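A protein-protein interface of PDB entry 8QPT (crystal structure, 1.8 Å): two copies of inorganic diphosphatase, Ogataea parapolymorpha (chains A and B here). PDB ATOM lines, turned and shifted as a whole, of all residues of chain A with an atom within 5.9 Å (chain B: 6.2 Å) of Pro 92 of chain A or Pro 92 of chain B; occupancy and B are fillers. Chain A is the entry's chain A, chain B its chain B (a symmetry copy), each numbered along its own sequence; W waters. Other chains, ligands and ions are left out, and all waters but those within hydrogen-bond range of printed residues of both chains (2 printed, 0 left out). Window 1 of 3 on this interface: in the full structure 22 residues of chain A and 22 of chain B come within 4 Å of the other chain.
The side-chain amide nitrogen (ND2) of Asn 193 of chain A is in hydrogen-bond range of the side-chain hydroxyl (OH) of Tyr 91 of chain B. A ring nitrogen (ND1) of His 94 of chain B sits at hydrogen-bond distance from a ring nitrogen (ND1) of His 94 of chain A (2.7 Å). OH of Tyr 91 of chain A lies within hydrogen-bond range of ND2 of Asn 193 of chain B (3.0 Å).
ND2 of Asn 93 of chain B is in hydrogen-bond range of O of Ile 90 of chain B. The side-chain amide oxygen (OD1) of Asn 93 of chain A lies within hydrogen-bond range of the side-chain amide nitrogen (ND2) of Asn 193 of chain A. The backbone carbonyl oxygen (O) of Asn 89 of chain B is in hydrogen-bond range of the backbone NH (N) of Ser 286 of chain B, at 2.8 Å. The backbone carbonyl oxygen (O) of Ile 90 of chain A sits at hydrogen-bond distance from the side-chain amide nitrogen (ND2) of Asn 93 of chain A. The backbone NH (N) of Tyr 91 of chain B sits at hydrogen-bond distance from the backbone carbonyl oxygen (O) of Ser 286 of chain B, at 2.9 Å. The side-chain amide nitrogen (ND2) of Asn 193 of chain B lies within hydrogen-bond range of the side-chain amide oxygen (OD1) of Asn 93 of chain B.
Among the printed residues, merely in contact across the chains: His 94 of chain A with Trp 59 of chain B, Trp 59 of chain A with His 94 of chain B, Pro 92 of chain A with Asn 93 of chain B, Asn 93 of chain A with Pro 92 of chain B, Pro 92 of chain A with Asn 193 of chain B, Asn 193 of chain A with Pro 92 of chain B, Trp 59 of chain A with Asn 89 of chain B and Pro 92 of chain A with Pro 92 of chain B.
Of chain B, only Pro 92, Asn 93 and Asn 193 come within 4 Å of Pro 92 of chain A. Pro 92 of chain B touches just these residues of chain A: Pro 92 (3.96 Å), Asn 93 (3.5 Å) and Asn 193 (3.5 Å). Printed residues of chain A within 4 Å of Asn 93 of chain B: Pro 92 (3.4 Å). Of the printed residues of chain A, Asn 193 of chain B touches Tyr 91 (3.0 Å) and Pro 92 (3.5 Å). Printed residues of chain B within 4 Å of Asn 93 of chain A: Pro 92. Of the printed residues of chain B, His 94 of chain A touches Trp 59 and His 94. Ser 286 of chain B touches none of the printed residues of chain A. The nearest printed residue of chain A that does not touch Asn 93 of chain B is Trp 59 of chain A (4.5 Å).
Printed residues of chain A that touch a printed residue of chain B: Trp 59, Tyr 91, Pro 92, Asn 93, His 94 and Asn 193. Hydrophobic or aromatic side chains of chain A that line the printed part of chain B: Trp 59, Tyr 91, Pro 92 and His 94. Of the 10 printed residues of chain B, 7 touch a printed residue of chain A. Among the printed residues, 11 pairs touch across the chains.
Trp 59 of chain A touches His 94 of chain B, and with the chains exchanged His 94 of chain A touches Trp 59 of chain B. Tyr 91 of chain A touches Asn 193 of chain B, and with the chains exchanged Asn 193 of chain A touches Tyr 91 of chain B. Pro 92 of chain A touches Asn 93 of chain B, and with the chains exchanged Asn 93 of chain A touches Pro 92 of chain B. Pro 92 of chain A touches Asn 193 of chain B, and with the chains exchanged Asn 193 of chain A touches Pro 92 of chain B. Positions printed for both chains: 59, 90, 91, 92, 93, 94, 97 and 193. Of the 11 pairs that touch across the chains among the printed residues, 10 have their exchanged pair printed and touching as well.
Water W2 lies within hydrogen-bond range of the backbone carbonyl oxygen (O) of Pro 92 of chain B (2.6 Å), the side-chain amide oxygen (OD1) of Asn 93 of chain A (2.8 Å) and the backbone NH (N) of His 94 of chain A (3.5 Å). Water W1 lies within hydrogen-bond range of O of Pro 92 of chain A (2.7 Å), OD1 of Asn 93 of chain B (2.9 Å), N of His 94 of chain B (3.3 Å) and NE1 of Trp 59 of chain B (3.5 Å).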
ATOM      1  N   TRP A  59     -35.102  -3.602  -3.442  1.00  0.00           N
ATOM      2  CA  TRP A  59     -34.577  -3.596  -2.047  1.00  0.00           C
ATOM      3  C   TRP A  59     -35.745  -3.503  -1.058  1.00  0.00           C
ATOM      4  O   TRP A  59     -35.537  -3.166   0.102  1.00  0.00           O
ATOM      5  CB  TRP A  59     -33.558  -2.487  -1.799  1.00  0.00           C
ATOM      6  CG  TRP A  59     -32.348  -2.663  -2.657  1.00  0.00           C
ATOM      7  CD1 TRP A  59     -31.757  -3.848  -3.017  1.00  0.00           C
ATOM      8  CD2 TRP A  59     -31.580  -1.600  -3.256  1.00  0.00           C
ATOM      9  NE1 TRP A  59     -30.646  -3.591  -3.782  1.00  0.00           N
ATOM     10  CE2 TRP A  59     -30.543  -2.230  -4.001  1.00  0.00           C
ATOM     11  CE3 TRP A  59     -31.750  -0.209  -3.325  1.00  0.00           C
ATOM     12  CZ2 TRP A  59     -29.631  -1.523  -4.724  1.00  0.00           C
ATOM     13  CZ3 TRP A  59     -30.814   0.498  -4.053  1.00  0.00           C
ATOM     14  CH2 TRP A  59     -29.770  -0.144  -4.699  1.00  0.00           C
ATOM     15  N   ILE A  90     -31.848 -12.979   0.633  1.00  0.00           N
ATOM     16  CA  ILE A  90     -30.994 -14.086   0.144  1.00  0.00           C
ATOM     17  C   ILE A  90     -29.600 -13.527   0.023  1.00  0.00           C
ATOM     18  O   ILE A  90     -29.316 -12.781  -0.969  1.00  0.00           O
ATOM     19  CB  ILE A  90     -31.562 -14.597  -1.176  1.00  0.00           C
ATOM     20  CG1 ILE A  90     -33.028 -15.020  -1.103  1.00  0.00           C
ATOM     21  CG2 ILE A  90     -30.606 -15.637  -1.739  1.00  0.00           C
ATOM     22  CD1 ILE A  90     -33.321 -15.974   0.050  1.00  0.00           C
ATOM     23  N   TYR A  91     -28.788 -13.759   1.032  1.00  0.00           N
ATOM     24  CA  TYR A  91     -27.542 -13.022   1.255  1.00  0.00           C
ATOM     25  C   TYR A  91     -26.741 -13.089  -0.011  1.00  0.00           C
ATOM     26  O   TYR A  91     -26.650 -14.155  -0.582  1.00  0.00           O
ATOM     27  CB  TYR A  91     -26.722 -13.613   2.404  1.00  0.00           C
ATOM     28  CG  TYR A  91     -25.427 -12.883   2.648  1.00  0.00           C
ATOM     29  CD1 TYR A  91     -25.442 -11.795   3.514  1.00  0.00           C
ATOM     30  CD2 TYR A  91     -24.237 -13.223   2.033  1.00  0.00           C
ATOM     31  CE1 TYR A  91     -24.311 -11.033   3.748  1.00  0.00           C
ATOM     32  CE2 TYR A  91     -23.086 -12.499   2.280  1.00  0.00           C
ATOM     33  CZ  TYR A  91     -23.128 -11.384   3.139  1.00  0.00           C
ATOM     34  OH  TYR A  91     -21.971 -10.755   3.409  1.00  0.00           O
ATOM     35  N   PRO A  92     -26.143 -11.985  -0.515  1.00  0.00           N
ATOM     36  CA  PRO A  92     -26.131 -10.672   0.146  1.00  0.00           C
ATOM     37  C   PRO A  92     -27.176  -9.693  -0.398  1.00  0.00           C
ATOM     38  O   PRO A  92     -27.068  -8.513  -0.143  1.00  0.00           O
ATOM     39  CB  PRO A  92     -24.699 -10.177  -0.193  1.00  0.00           C
ATOM     40  CG  PRO A  92     -24.389 -10.794  -1.558  1.00  0.00           C
ATOM     41  CD  PRO A  92     -25.230 -12.068  -1.645  1.00  0.00           C
ATOM     42  N   ASN A  93     -28.235 -10.198  -1.035  1.00  0.00           N
ATOM     43  CA  ASN A  93     -29.420  -9.428  -1.467  1.00  0.00           C
ATOM     44  C   ASN A  93     -30.117  -8.811  -0.272  1.00  0.00           C
ATOM     45  O   ASN A  93     -30.189  -9.423   0.805  1.00  0.00           O
ATOM     46  CB  ASN A  93     -30.413 -10.243  -2.298  1.00  0.00           C
ATOM     47  CG  ASN A  93     -29.801 -10.656  -3.617  1.00  0.00           C
ATOM     48  OD1 ASN A  93     -29.641  -9.835  -4.523  1.00  0.00           O
ATOM     49  ND2 ASN A  93     -29.341 -11.874  -3.730  1.00  0.00           N
ATOM     50  N   HIS A  94     -30.582  -7.584  -0.461  1.00  0.00           N
ATOM     51  CA  HIS A  94     -31.542  -6.942   0.435  1.00  0.00           C
ATOM     52  C   HIS A  94     -32.883  -6.938  -0.268  1.00  0.00           C
ATOM     53  O   HIS A  94     -33.071  -6.183  -1.258  1.00  0.00           O
ATOM     54  CB  HIS A  94     -31.095  -5.498   0.759  1.00  0.00           C
ATOM     55  CG  HIS A  94     -31.987  -4.776   1.719  1.00  0.00           C
ATOM     56  ND1 HIS A  94     -31.980  -3.379   1.821  1.00  0.00           N
ATOM     57  CD2 HIS A  94     -32.824  -5.239   2.670  1.00  0.00           C
ATOM     58  CE1 HIS A  94     -32.849  -3.015   2.789  1.00  0.00           C
ATOM     59  NE2 HIS A  94     -33.365  -4.142   3.312  1.00  0.00           N
ATOM     60  N   PRO A  97     -33.832  -7.951  -5.669  1.00  0.00           N
ATOM     61  CA  PRO A  97     -32.592  -7.317  -6.148  1.00  0.00           C
ATOM     62  C   PRO A  97     -32.798  -6.299  -7.281  1.00  0.00           C
ATOM     63  O   PRO A  97     -31.905  -5.562  -7.582  1.00  0.00           O
ATOM     64  CB  PRO A  97     -31.790  -8.513  -6.628  1.00  0.00           C
ATOM     65  CG  PRO A  97     -32.878  -9.526  -7.083  1.00  0.00           C
ATOM     66  CD  PRO A  97     -33.916  -9.393  -5.980  1.00  0.00           C
ATOM     67  N   ASN A 193     -27.152 -13.636 -10.553  1.00  0.00           N
ATOM     68  CA  ASN A 193     -27.779 -13.412  -9.230  1.00  0.00           C
ATOM     69  C   ASN A 193     -29.291 -13.683  -9.330  1.00  0.00           C
ATOM     70  O   ASN A 193     -29.859 -14.266  -8.376  1.00  0.00           O
ATOM     71  CB  ASN A 193     -27.493 -12.012  -8.671  1.00  0.00           C
ATOM     72  CG  ASN A 193     -28.212 -11.740  -7.373  1.00  0.00           C
ATOM     73  OD1 ASN A 193     -27.936 -12.371  -6.352  1.00  0.00           O
ATOM     74  ND2 ASN A 193     -28.894 -10.611  -7.330  1.00  0.00           N
ATOM     75  N   TRP B  59     -27.024  -1.856   5.232  1.00  0.00           N
ATOM     76  CA  TRP B  59     -27.824  -1.517   4.035  1.00  0.00           C
ATOM     77  C   TRP B  59     -27.958   0.004   3.977  1.00  0.00           C
ATOM     78  O   TRP B  59     -28.811   0.440   3.168  1.00  0.00           O
ATOM     79  CB  TRP B  59     -29.175  -2.217   3.985  1.00  0.00           C
ATOM     80  CG  TRP B  59     -29.004  -3.705   3.951  1.00  0.00           C
ATOM     81  CD1 TRP B  59     -28.104  -4.403   3.192  1.00  0.00           C
ATOM     82  CD2 TRP B  59     -29.832  -4.687   4.605  1.00  0.00           C
ATOM     83  NE1 TRP B  59     -28.257  -5.751   3.394  1.00  0.00           N
ATOM     84  CE2 TRP B  59     -29.327  -5.950   4.235  1.00  0.00           C
ATOM     85  CE3 TRP B  59     -30.930  -4.610   5.477  1.00  0.00           C
ATOM     86  CZ2 TRP B  59     -29.893  -7.127   4.705  1.00  0.00           C
ATOM     87  CZ3 TRP B  59     -31.468  -5.786   5.970  1.00  0.00           C
ATOM     88  CH2 TRP B  59     -30.946  -7.023   5.584  1.00  0.00           C
ATOM     89  N   ASN B  89     -23.204   0.717  -4.371  1.00  0.00           N
ATOM     90  CA  ASN B  89     -23.946  -0.583  -4.244  1.00  0.00           C
ATOM     91  C   ASN B  89     -23.168  -1.543  -5.117  1.00  0.00           C
ATOM     92  O   ASN B  89     -23.333  -1.515  -6.371  1.00  0.00           O
ATOM     93  CB  ASN B  89     -25.408  -0.455  -4.676  1.00  0.00           C
ATOM     94  CG  ASN B  89     -26.127   0.581  -3.862  1.00  0.00           C
ATOM     95  OD1 ASN B  89     -26.207   0.451  -2.659  1.00  0.00           O
ATOM     96  ND2 ASN B  89     -26.556   1.680  -4.465  1.00  0.00           N
ATOM     97  N   ILE B  90     -22.265  -2.310  -4.507  1.00  0.00           N
ATOM     98  CA  ILE B  90     -21.429  -3.313  -5.172  1.00  0.00           C
ATOM     99  C   ILE B  90     -22.282  -4.552  -5.452  1.00  0.00           C
ATOM    100  O   ILE B  90     -22.541  -5.332  -4.533  1.00  0.00           O
ATOM    101  CB  ILE B  90     -20.193  -3.596  -4.334  1.00  0.00           C
ATOM    102  CG1 ILE B  90     -19.430  -2.292  -4.045  1.00  0.00           C
ATOM    103  CG2 ILE B  90     -19.388  -4.683  -5.022  1.00  0.00           C
ATOM    104  CD1 ILE B  90     -19.080  -1.403  -5.252  1.00  0.00           C
ATOM    105  N   TYR B  91     -22.839  -4.598  -6.651  1.00  0.00           N
ATOM    106  CA  TYR B  91     -23.965  -5.507  -6.953  1.00  0.00           C
ATOM    107  C   TYR B  91     -23.602  -6.920  -6.487  1.00  0.00           C
ATOM    108  O   TYR B  91     -22.496  -7.398  -6.794  1.00  0.00           O
ATOM    109  CB  TYR B  91     -24.247  -5.573  -8.454  1.00  0.00           C
ATOM    110  CG  TYR B  91     -25.445  -6.450  -8.759  1.00  0.00           C
ATOM    111  CD1 TYR B  91     -26.713  -5.937  -8.706  1.00  0.00           C
ATOM    112  CD2 TYR B  91     -25.319  -7.808  -9.076  1.00  0.00           C
ATOM    113  CE1 TYR B  91     -27.797  -6.709  -8.975  1.00  0.00           C
ATOM    114  CE2 TYR B  91     -26.391  -8.566  -9.415  1.00  0.00           C
ATOM    115  CZ  TYR B  91     -27.661  -8.058  -9.292  1.00  0.00           C
ATOM    116  OH  TYR B  91     -28.755  -8.792  -9.681  1.00  0.00           O
ATOM    117  N   PRO B  92     -24.481  -7.657  -5.795  1.00  0.00           N
ATOM    118  CA  PRO B  92     -25.848  -7.267  -5.469  1.00  0.00           C
ATOM    119  C   PRO B  92     -26.096  -6.687  -4.077  1.00  0.00           C
ATOM    120  O   PRO B  92     -27.234  -6.596  -3.606  1.00  0.00           O
ATOM    121  CB  PRO B  92     -26.593  -8.614  -5.603  1.00  0.00           C
ATOM    122  CG  PRO B  92     -25.589  -9.645  -5.203  1.00  0.00           C
ATOM    123  CD  PRO B  92     -24.214  -9.078  -5.494  1.00  0.00           C
ATOM    124  N   ASN B  93     -25.028  -6.208  -3.458  1.00  0.00           N
ATOM    125  CA  ASN B  93     -25.122  -5.573  -2.157  1.00  0.00           C
ATOM    126  C   ASN B  93     -25.921  -4.268  -2.255  1.00  0.00           C
ATOM    127  O   ASN B  93     -25.901  -3.570  -3.307  1.00  0.00           O
ATOM    128  CB  ASN B  93     -23.736  -5.222  -1.616  1.00  0.00           C
ATOM    129  CG  ASN B  93     -22.943  -6.453  -1.260  1.00  0.00           C
ATOM    130  OD1 ASN B  93     -23.234  -7.061  -0.252  1.00  0.00           O
ATOM    131  ND2 ASN B  93     -22.041  -6.871  -2.121  1.00  0.00           N
ATOM    132  N   HIS B  94     -26.583  -3.988  -1.134  1.00  0.00           N
ATOM    133  CA  HIS B  94     -27.256  -2.704  -0.918  1.00  0.00           C
ATOM    134  C   HIS B  94     -26.505  -1.974   0.154  1.00  0.00           C
ATOM    135  O   HIS B  94     -26.565  -2.350   1.282  1.00  0.00           O
ATOM    136  CB  HIS B  94     -28.728  -2.854  -0.581  1.00  0.00           C
ATOM    137  CG  HIS B  94     -29.464  -1.559  -0.426  1.00  0.00           C
ATOM    138  ND1 HIS B  94     -30.592  -1.500   0.412  1.00  0.00           N
ATOM    139  CD2 HIS B  94     -29.225  -0.272  -0.893  1.00  0.00           C
ATOM    140  CE1 HIS B  94     -31.068  -0.216   0.363  1.00  0.00           C
ATOM    141  NE2 HIS B  94     -30.246   0.590  -0.425  1.00  0.00           N
ATOM    142  N   PRO B  97     -22.821  -4.276   3.602  1.00  0.00           N
ATOM    143  CA  PRO B  97     -23.541  -5.553   3.726  1.00  0.00           C
ATOM    144  C   PRO B  97     -23.849  -5.976   5.168  1.00  0.00           C
ATOM    145  O   PRO B  97     -24.544  -6.952   5.354  1.00  0.00           O
ATOM    146  CB  PRO B  97     -22.600  -6.518   2.981  1.00  0.00           C
ATOM    147  CG  PRO B  97     -21.241  -5.890   3.124  1.00  0.00           C
ATOM    148  CD  PRO B  97     -21.466  -4.409   3.016  1.00  0.00           C
ATOM    149  N   ASN B 193     -18.188 -12.629   0.324  1.00  0.00           N
ATOM    150  CA  ASN B 193     -18.776 -11.315  -0.056  1.00  0.00           C
ATOM    151  C   ASN B 193     -17.935 -10.173   0.544  1.00  0.00           C
ATOM    152  O   ASN B 193     -17.692  -9.195  -0.170  1.00  0.00           O
ATOM    153  CB  ASN B 193     -20.258 -11.308   0.249  1.00  0.00           C
ATOM    154  CG  ASN B 193     -20.880  -9.956  -0.106  1.00  0.00           C
ATOM    155  OD1 ASN B 193     -20.848  -9.575  -1.251  1.00  0.00           O
ATOM    156  ND2 ASN B 193     -21.514  -9.265   0.820  1.00  0.00           N
ATOM    157  N   SER B 286     -23.450  -0.749  -9.053  1.00  0.00           N
ATOM    158  CA  SER B 286     -22.114  -0.954  -9.681  1.00  0.00           C
ATOM    159  C   SER B 286     -21.933  -2.417  -9.971  1.00  0.00           C
ATOM    160  O   SER B 286     -21.966  -3.263  -9.039  1.00  0.00           O
ATOM    161  CB  SER B 286     -21.027  -0.423  -8.784  1.00  0.00           C
ATOM    162  OG  SER B 286     -21.258   0.947  -8.509  1.00  0.00           O
HETATM  163  O   HOH W   1     -25.815  -6.429   1.005  1.00  0.00           O
HETATM  164  O   HOH W   2     -29.813  -7.124  -3.803  1.00  0.00           O
